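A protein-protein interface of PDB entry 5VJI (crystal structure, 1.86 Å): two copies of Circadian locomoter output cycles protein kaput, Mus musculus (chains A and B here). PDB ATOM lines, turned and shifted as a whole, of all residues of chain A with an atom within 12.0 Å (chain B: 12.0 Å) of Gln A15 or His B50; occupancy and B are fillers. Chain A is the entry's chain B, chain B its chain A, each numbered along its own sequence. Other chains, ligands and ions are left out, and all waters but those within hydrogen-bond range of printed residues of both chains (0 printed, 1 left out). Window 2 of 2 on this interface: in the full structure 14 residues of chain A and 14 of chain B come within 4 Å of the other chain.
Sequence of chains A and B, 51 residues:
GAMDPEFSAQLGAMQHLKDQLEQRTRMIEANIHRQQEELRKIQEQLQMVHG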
ATOM      1  N   PHE A   7      -3.248  13.909  -6.658  1.00  0.00           N
ATOM      2  CA  PHE A   7      -2.777  13.895  -5.269  1.00  0.00           C
ATOM      3  C   PHE A   7      -2.746  15.319  -4.730  1.00  0.00           C
ATOM      4  O   PHE A   7      -2.965  15.547  -3.552  1.00  0.00           O
ATOM      5  CB  PHE A   7      -1.399  13.247  -5.157  1.00  0.00           C
ATOM      6  N   SER A   8      -2.471  16.273  -5.620  1.00  0.00           N
ATOM      7  CA  SER A   8      -2.793  17.667  -5.341  1.00  0.00           C
ATOM      8  C   SER A   8      -4.282  17.828  -5.079  1.00  0.00           C
ATOM      9  O   SER A   8      -4.685  18.561  -4.167  1.00  0.00           O
ATOM     10  CB  SER A   8      -2.385  18.542  -6.522  1.00  0.00           C
ATOM     11  OG  SER A   8      -3.174  18.207  -7.659  1.00  0.00           O
ATOM     12  N   ALA A   9      -5.118  17.142  -5.876  1.00  0.00           N
ATOM     13  CA  ALA A   9      -6.562  17.215  -5.694  1.00  0.00           C
ATOM     14  C   ALA A   9      -6.985  16.701  -4.320  1.00  0.00           C
ATOM     15  O   ALA A   9      -7.873  17.279  -3.675  1.00  0.00           O
ATOM     16  CB  ALA A   9      -7.262  16.426  -6.795  1.00  0.00           C
ATOM     17  N   GLN A  10      -6.362  15.618  -3.849  1.00  0.00           N
ATOM     18  CA  GLN A  10      -6.741  15.087  -2.550  1.00  0.00           C
ATOM     19  C   GLN A  10      -6.320  16.033  -1.436  1.00  0.00           C
ATOM     20  O   GLN A  10      -7.082  16.264  -0.497  1.00  0.00           O
ATOM     21  CB  GLN A  10      -6.130  13.709  -2.339  1.00  0.00           C
ATOM     22  CG  GLN A  10      -6.907  12.603  -2.997  1.00  0.00           C
ATOM     23  CD  GLN A  10      -6.011  11.699  -3.821  1.00  0.00           C
ATOM     24  OE1 GLN A  10      -4.803  11.612  -3.579  1.00  0.00           O
ATOM     25  NE2 GLN A  10      -6.595  11.032  -4.815  1.00  0.00           N
ATOM     26  N   LEU A  11      -5.110  16.589  -1.530  1.00  0.00           N
ATOM     27  CA  LEU A  11      -4.663  17.551  -0.534  1.00  0.00           C
ATOM     28  C   LEU A  11      -5.632  18.717  -0.423  1.00  0.00           C
ATOM     29  O   LEU A  11      -5.970  19.146   0.686  1.00  0.00           O
ATOM     30  CB  LEU A  11      -3.259  18.041  -0.877  1.00  0.00           C
ATOM     31  CG  LEU A  11      -2.127  17.327  -0.131  1.00  0.00           C
ATOM     32  CD1 LEU A  11      -2.516  15.884   0.261  1.00  0.00           C
ATOM     33  CD2 LEU A  11      -0.849  17.342  -0.973  1.00  0.00           C
ATOM     34  N   GLY A  12      -6.120  19.229  -1.554  1.00  0.00           N
ATOM     35  CA  GLY A  12      -7.061  20.342  -1.489  1.00  0.00           C
ATOM     36  C   GLY A  12      -8.412  19.972  -0.896  1.00  0.00           C
ATOM     37  O   GLY A  12      -9.050  20.791  -0.224  1.00  0.00           O
ATOM     38  N   ALA A  13      -8.883  18.749  -1.149  1.00  0.00           N
ATOM     39  CA  ALA A  13     -10.143  18.330  -0.545  1.00  0.00           C
ATOM     40  C   ALA A  13     -10.015  18.208   0.972  1.00  0.00           C
ATOM     41  O   ALA A  13     -10.887  18.656   1.712  1.00  0.00           O
ATOM     42  CB  ALA A  13     -10.579  17.005  -1.133  1.00  0.00           C
ATOM     43  N   MET A  14      -8.953  17.560   1.448  1.00  0.00           N
ATOM     44  CA  MET A  14      -8.804  17.406   2.891  1.00  0.00           C
ATOM     45  C   MET A  14      -8.559  18.776   3.530  1.00  0.00           C
ATOM     46  O   MET A  14      -9.056  19.012   4.620  1.00  0.00           O
ATOM     47  CB  MET A  14      -7.682  16.411   3.244  1.00  0.00           C
ATOM     48  CG  MET A  14      -7.963  14.928   2.840  1.00  0.00           C
ATOM     49  SD  MET A  14      -9.431  13.925   3.741  1.00  0.00           S
ATOM     50  CE  MET A  14      -8.987  12.110   3.151  1.00  0.00           C
ATOM     51  N   GLN A  15      -7.828  19.668   2.837  1.00  0.00           N
ATOM     52  CA  GLN A  15      -7.623  21.016   3.359  1.00  0.00           C
ATOM     53  C   GLN A  15      -8.920  21.815   3.403  1.00  0.00           C
ATOM     54  O   GLN A  15      -9.084  22.654   4.294  1.00  0.00           O
ATOM     55  CB  GLN A  15      -6.574  21.754   2.522  1.00  0.00           C
ATOM     56  CG  GLN A  15      -6.249  23.153   2.991  1.00  0.00           C
ATOM     57  CD  GLN A  15      -5.292  23.160   4.176  1.00  0.00           C
ATOM     58  OE1 GLN A  15      -4.590  22.168   4.430  1.00  0.00           O
ATOM     59  NE2 GLN A  15      -5.260  24.276   4.913  1.00  0.00           N
ATOM     60  N   HIS A  16      -9.843  21.588   2.461  1.00  0.00           N
ATOM     61  CA  HIS A  16     -11.170  22.189   2.581  1.00  0.00           C
ATOM     62  C   HIS A  16     -11.884  21.684   3.835  1.00  0.00           C
ATOM     63  O   HIS A  16     -12.436  22.482   4.582  1.00  0.00           O
ATOM     64  CB  HIS A  16     -12.029  21.938   1.335  1.00  0.00           C
ATOM     65  CG  HIS A  16     -13.413  22.503   1.456  1.00  0.00           C
ATOM     66  ND1 HIS A  16     -13.741  23.774   1.043  1.00  0.00           N
ATOM     67  CD2 HIS A  16     -14.532  21.995   2.024  1.00  0.00           C
ATOM     68  CE1 HIS A  16     -15.010  24.020   1.329  1.00  0.00           C
ATOM     69  NE2 HIS A  16     -15.510  22.956   1.926  1.00  0.00           N
ATOM     70  N   LEU A  17     -11.799  20.382   4.133  1.00  0.00           N
ATOM     71  CA  LEU A  17     -12.409  19.837   5.353  1.00  0.00           C
ATOM     72  C   LEU A  17     -11.774  20.439   6.595  1.00  0.00           C
ATOM     73  O   LEU A  17     -12.465  20.876   7.519  1.00  0.00           O
ATOM     74  CB  LEU A  17     -12.253  18.320   5.393  1.00  0.00           C
ATOM     75  CG  LEU A  17     -13.274  17.592   4.510  1.00  0.00           C
ATOM     76  CD1 LEU A  17     -12.936  16.134   4.249  1.00  0.00           C
ATOM     77  CD2 LEU A  17     -14.670  17.699   5.138  1.00  0.00           C
ATOM     78  N   LYS A  18     -10.452  20.423   6.639  1.00  0.00           N
ATOM     79  CA  LYS A  18      -9.702  20.977   7.753  1.00  0.00           C
ATOM     80  C   LYS A  18     -10.091  22.428   7.988  1.00  0.00           C
ATOM     81  O   LYS A  18     -10.351  22.831   9.134  1.00  0.00           O
ATOM     82  CB  LYS A  18      -8.204  20.830   7.436  1.00  0.00           C
ATOM     83  CG  LYS A  18      -7.216  21.400   8.468  1.00  0.00           C
ATOM     84  CD  LYS A  18      -5.794  21.323   7.865  1.00  0.00           C
ATOM     85  CE  LYS A  18      -4.726  22.091   8.642  1.00  0.00           C
ATOM     86  NZ  LYS A  18      -3.434  21.287   8.537  1.00  0.00           N
ATOM     87  N   ASP A  19     -10.233  23.205   6.907  1.00  0.00           N
ATOM     88  CA  ASP A  19     -10.523  24.627   7.061  1.00  0.00           C
ATOM     89  C   ASP A  19     -11.918  24.870   7.612  1.00  0.00           C
ATOM     90  O   ASP A  19     -12.122  25.831   8.353  1.00  0.00           O
ATOM     91  CB  ASP A  19     -10.330  25.368   5.743  1.00  0.00           C
ATOM     92  CG  ASP A  19      -8.852  25.525   5.376  1.00  0.00           C
ATOM     93  OD1 ASP A  19      -8.000  25.457   6.290  1.00  0.00           O
ATOM     94  OD2 ASP A  19      -8.535  25.732   4.180  1.00  0.00           O
ATOM     95  N   GLN A  20     -12.888  24.023   7.265  1.00  0.00           N
ATOM     96  CA  GLN A  20     -14.230  24.186   7.814  1.00  0.00           C
ATOM     97  C   GLN A  20     -14.259  23.825   9.297  1.00  0.00           C
ATOM     98  O   GLN A  20     -14.885  24.537  10.084  1.00  0.00           O
ATOM     99  CB  GLN A  20     -15.244  23.346   7.032  1.00  0.00           C
ATOM    100  CG  GLN A  20     -15.280  23.628   5.547  1.00  0.00           C
ATOM    101  CD  GLN A  20     -16.218  24.765   5.191  1.00  0.00           C
ATOM    102  OE1 GLN A  20     -16.186  25.829   5.814  1.00  0.00           O
ATOM    103  NE2 GLN A  20     -17.065  24.542   4.177  1.00  0.00           N
ATOM    104  N   LEU A  21     -13.583  22.735   9.704  1.00  0.00           N
ATOM    105  CA  LEU A  21     -13.452  22.415  11.134  1.00  0.00           C
ATOM    106  C   LEU A  21     -12.716  23.525  11.901  1.00  0.00           C
ATOM    107  O   LEU A  21     -13.115  23.872  13.013  1.00  0.00           O
ATOM    108  CB  LEU A  21     -12.720  21.090  11.351  1.00  0.00           C
ATOM    109  CG  LEU A  21     -13.474  19.894  10.745  1.00  0.00           C
ATOM    110  CD1 LEU A  21     -12.522  18.740  10.593  1.00  0.00           C
ATOM    111  CD2 LEU A  21     -14.706  19.512  11.570  1.00  0.00           C
ATOM    112  N   GLU A  22     -11.617  24.063  11.346  1.00  0.00           N
ATOM    113  CA  GLU A  22     -10.955  25.185  12.014  1.00  0.00           C
ATOM    114  C   GLU A  22     -11.903  26.374  12.152  1.00  0.00           C
ATOM    115  O   GLU A  22     -11.907  27.061  13.191  1.00  0.00           O
ATOM    116  CB  GLU A  22      -9.663  25.584  11.268  1.00  0.00           C
ATOM    117  CG  GLU A  22      -8.525  24.618  11.513  1.00  0.00           C
ATOM    118  CD  GLU A  22      -7.284  24.909  10.701  1.00  0.00           C
ATOM    119  OE1 GLU A  22      -7.306  25.849   9.873  1.00  0.00           O
ATOM    120  OE2 GLU A  22      -6.282  24.182  10.890  1.00  0.00           O
ATOM    121  N   GLN A  23     -12.692  26.655  11.111  1.00  0.00           N
ATOM    122  CA  GLN A  23     -13.680  27.715  11.197  1.00  0.00           C
ATOM    123  C   GLN A  23     -14.662  27.455  12.332  1.00  0.00           C
ATOM    124  O   GLN A  23     -15.002  28.386  13.063  1.00  0.00           O
ATOM    125  CB  GLN A  23     -14.437  27.892   9.879  1.00  0.00           C
ATOM    126  CG  GLN A  23     -15.512  28.963   9.868  1.00  0.00           C
ATOM    127  CD  GLN A  23     -14.982  30.364  10.169  1.00  0.00           C
ATOM    128  OE1 GLN A  23     -13.862  30.725   9.785  1.00  0.00           O
ATOM    129  NE2 GLN A  23     -15.793  31.159  10.870  1.00  0.00           N
ATOM    130  N   ARG A  24     -15.100  26.197  12.513  1.00  0.00           N
ATOM    131  CA  ARG A  24     -15.968  25.879  13.656  1.00  0.00           C
ATOM    132  C   ARG A  24     -15.292  26.206  14.984  1.00  0.00           C
ATOM    133  O   ARG A  24     -15.929  26.751  15.886  1.00  0.00           O
ATOM    134  CB  ARG A  24     -16.385  24.395  13.636  1.00  0.00           C
ATOM    135  CG  ARG A  24     -17.379  24.065  12.530  1.00  0.00           C
ATOM    136  CD  ARG A  24     -18.726  24.668  12.826  1.00  0.00           C
ATOM    137  NE  ARG A  24     -19.314  24.056  14.023  1.00  0.00           N
ATOM    138  CZ  ARG A  24     -19.880  24.719  15.029  1.00  0.00           C
ATOM    139  NH1 ARG A  24     -20.366  24.029  16.044  1.00  0.00           N
ATOM    140  NH2 ARG A  24     -19.958  26.060  15.021  1.00  0.00           N
ATOM    141  N   ARG A  26     -13.259  28.536  15.588  1.00  0.00           N
ATOM    142  CA  ARG A  26     -13.231  29.971  15.785  1.00  0.00           C
ATOM    143  C   ARG A  26     -14.596  30.533  16.165  1.00  0.00           C
ATOM    144  O   ARG A  26     -14.654  31.520  16.911  1.00  0.00           O
ATOM    145  CB  ARG A  26     -12.710  30.660  14.528  1.00  0.00           C
ATOM    146  CG  ARG A  26     -11.250  30.384  14.263  1.00  0.00           C
ATOM    147  CD  ARG A  26     -10.677  31.367  13.221  1.00  0.00           C
ATOM    148  NE  ARG A  26     -11.177  31.160  11.863  1.00  0.00           N
ATOM    149  CZ  ARG A  26     -10.668  30.281  10.999  1.00  0.00           C
ATOM    150  NH1 ARG A  26      -9.665  29.502  11.365  1.00  0.00           N
ATOM    151  NH2 ARG A  26     -11.169  30.175   9.772  1.00  0.00           N
ATOM    152  N   ILE B  42      -8.338  20.571  19.823  1.00  0.00           N
ATOM    153  CA  ILE B  42      -8.870  20.323  18.490  1.00  0.00           C
ATOM    154  C   ILE B  42      -8.047  21.065  17.441  1.00  0.00           C
ATOM    155  O   ILE B  42      -7.764  20.525  16.373  1.00  0.00           O
ATOM    156  CB  ILE B  42     -10.353  20.737  18.415  1.00  0.00           C
ATOM    157  CG1 ILE B  42     -11.227  19.832  19.284  1.00  0.00           C
ATOM    158  CG2 ILE B  42     -10.825  20.802  16.931  1.00  0.00           C
ATOM    159  CD1 ILE B  42     -12.623  20.447  19.538  1.00  0.00           C
ATOM    160  N   GLN B  43      -7.683  22.331  17.723  1.00  0.00           N
ATOM    161  CA  GLN B  43      -6.890  23.102  16.769  1.00  0.00           C
ATOM    162  C   GLN B  43      -5.526  22.435  16.557  1.00  0.00           C
ATOM    163  O   GLN B  43      -5.050  22.305  15.426  1.00  0.00           O
ATOM    164  CB  GLN B  43      -6.756  24.560  17.271  1.00  0.00           C
ATOM    165  CG  GLN B  43      -8.054  25.342  17.090  1.00  0.00           C
ATOM    166  CD  GLN B  43      -7.999  26.768  17.624  1.00  0.00           C
ATOM    167  OE1 GLN B  43      -7.106  27.118  18.399  1.00  0.00           O
ATOM    168  NE2 GLN B  43      -8.977  27.585  17.229  1.00  0.00           N
ATOM    169  N   GLU B  44      -4.922  21.931  17.637  1.00  0.00           N
ATOM    170  CA  GLU B  44      -3.606  21.292  17.555  1.00  0.00           C
ATOM    171  C   GLU B  44      -3.652  20.028  16.694  1.00  0.00           C
ATOM    172  O   GLU B  44      -2.744  19.779  15.889  1.00  0.00           O
ATOM    173  CB  GLU B  44      -3.138  20.948  18.976  1.00  0.00           C
ATOM    174  CG  GLU B  44      -1.675  21.196  19.330  1.00  0.00           C
ATOM    175  CD  GLU B  44      -1.461  21.246  20.867  1.00  0.00           C
ATOM    176  OE1 GLU B  44      -2.022  20.382  21.584  1.00  0.00           O
ATOM    177  OE2 GLU B  44      -0.760  22.164  21.356  1.00  0.00           O
ATOM    178  N   GLN B  45      -4.699  19.222  16.865  1.00  0.00           N
ATOM    179  CA  GLN B  45      -4.909  18.011  16.061  1.00  0.00           C
ATOM    180  C   GLN B  45      -5.088  18.335  14.574  1.00  0.00           C
ATOM    181  O   GLN B  45      -4.549  17.631  13.706  1.00  0.00           O
ATOM    182  CB  GLN B  45      -6.138  17.248  16.595  1.00  0.00           C
ATOM    183  CG  GLN B  45      -5.926  16.651  17.957  1.00  0.00           C
ATOM    184  CD  GLN B  45      -6.745  15.389  18.194  1.00  0.00           C
ATOM    185  OE1 GLN B  45      -7.950  15.339  17.919  1.00  0.00           O
ATOM    186  NE2 GLN B  45      -6.081  14.352  18.703  1.00  0.00           N
ATOM    187  N   LEU B  46      -5.863  19.388  14.264  1.00  0.00           N
ATOM    188  CA  LEU B  46      -6.094  19.748  12.860  1.00  0.00           C
ATOM    189  C   LEU B  46      -4.810  20.205  12.190  1.00  0.00           C
ATOM    190  O   LEU B  46      -4.590  19.938  10.999  1.00  0.00           O
ATOM    191  CB  LEU B  46      -7.147  20.853  12.742  1.00  0.00           C
ATOM    192  CG  LEU B  46      -8.567  20.426  13.104  1.00  0.00           C
ATOM    193  CD1 LEU B  46      -9.498  21.621  13.165  1.00  0.00           C
ATOM    194  CD2 LEU B  46      -9.049  19.398  12.098  1.00  0.00           C
ATOM    195  N   GLN B  47      -3.959  20.909  12.921  1.00  0.00           N
ATOM    196  CA  GLN B  47      -2.734  21.360  12.265  1.00  0.00           C
ATOM    197  C   GLN B  47      -1.777  20.220  11.940  1.00  0.00           C
ATOM    198  O   GLN B  47      -0.810  20.438  11.203  1.00  0.00           O
ATOM    199  CB  GLN B  47      -2.018  22.412  13.113  1.00  0.00           C
ATOM    200  CG  GLN B  47      -2.836  23.668  13.421  1.00  0.00           C
ATOM    201  CD  GLN B  47      -3.217  24.503  12.195  1.00  0.00           C
ATOM    202  OE1 GLN B  47      -4.174  25.278  12.240  1.00  0.00           O
ATOM    203  NE2 GLN B  47      -2.462  24.368  11.114  1.00  0.00           N
ATOM    204  N   MET B  48      -2.009  19.016  12.444  1.00  0.00           N
ATOM    205  CA  MET B  48      -1.149  17.864  12.153  1.00  0.00           C
ATOM    206  C   MET B  48      -1.441  17.283  10.766  1.00  0.00           C
ATOM    207  O   MET B  48      -0.621  16.559  10.203  1.00  0.00           O
ATOM    208  CB  MET B  48      -1.310  16.765  13.222  1.00  0.00           C
ATOM    209  CG  MET B  48      -0.676  17.075  14.586  1.00  0.00           C
ATOM    210  SD  MET B  48      -0.839  15.641  15.938  1.00  0.00           S
ATOM    211  CE  MET B  48      -0.295  16.637  17.529  1.00  0.00           C
ATOM    212  N   VAL B  49      -2.629  17.591  10.221  1.00  0.00           N
ATOM    213  CA  VAL B  49      -3.031  17.142   8.884  1.00  0.00           C
ATOM    214  C   VAL B  49      -2.255  17.909   7.817  1.00  0.00           C
ATOM    215  O   VAL B  49      -1.914  19.090   7.988  1.00  0.00           O
ATOM    216  CB  VAL B  49      -4.549  17.327   8.686  1.00  0.00           C
ATOM    217  CG1 VAL B  49      -4.987  16.767   7.367  1.00  0.00           C
ATOM    218  CG2 VAL B  49      -5.311  16.660   9.809  1.00  0.00           C
ATOM    219  N   HIS B  50      -1.995  17.245   6.690  1.00  0.00           N
ATOM    220  CA  HIS B  50      -1.418  17.908   5.520  1.00  0.00           C
ATOM    221  C   HIS B  50      -2.506  18.308   4.524  1.00  0.00           C
ATOM    222  O   HIS B  50      -3.672  18.504   4.888  1.00  0.00           O
ATOM    223  CB  HIS B  50      -0.391  17.008   4.831  1.00  0.00           C
ATOM    224  CG  HIS B  50       0.699  16.527   5.736  1.00  0.00           C
ATOM    225  ND1 HIS B  50       0.734  16.819   7.083  1.00  0.00           N
ATOM    226  CD2 HIS B  50       1.794  15.771   5.488  1.00  0.00           C
ATOM    227  CE1 HIS B  50       1.801  16.259   7.626  1.00  0.00           C
ATOM    228  NE2 HIS B  50       2.462  15.618   6.679  1.00  0.00           N
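Printed residues of chain B that touch a printed residue of chain A: Leu B46, Gln B47, Val B49 and His B50.
Hydrophobic or aromatic side chains of chain B that line the printed part of chain A: Leu B46.
Hydrophobic or aromatic side chains of chain A within 4 Å of the printed part of chain B: Leu A21.
Among the printed residues, no Asp or Glu carboxylate lies within 4 Å of a Lys or Arg side-chain nitrogen of the other chain.
O of Val B49 lies within hydrogen-bond range of NZ of Lys A18, at 2.7 Å.
OE2 of Glu A22 lies close to OE1 of Gln B47.
NZ of Lys A18 sits at hydrogen-bond distance from O of Leu B46, 3.0 Å away.
No position is printed for both chains.
His B50 touches Gln A15.
Gln B47 touches Lys A18.
CB of Leu A21 touches CD1 of Leu B46 (3.7 Å).
Glu A22 touches Leu B46.
The side-chain amide nitrogen of Gln A15 lies within hydrogen-bond range of the side-chain carboxylate of Asp A19 (3.3 Å).
The backbone carbonyl oxygen of Met B48 sits at hydrogen-bond distance from a ring nitrogen (ND1) of His B50 (3.4 Å).
No residue of chain B comes within 4 Å of Gly A12.
No residue of chain B comes within 4 Å of Ala A13.
Gln A15 touches just one residue of chain B: His B50.
No residue of chain B comes within 4 Å of His A16.
No residue of chain B comes within 4 Å of Leu A17.
Of the printed residues of chain B, Leu A21 touches Leu B46.
Of the printed residues of chain B, Glu A22 touches Leu B46 and Gln B47.
Of the printed residues of chain A, Leu B46 touches Lys A18, Leu A21 and Glu A22.
Of the printed residues of chain A, Gln B47 touches Lys A18 (3.8 Å) and Glu A22 (2.7 Å).
Of the printed residues of chain A, Val B49 touches Lys A18.
Of the printed residues of chain A, His B50 touches Gln A15.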
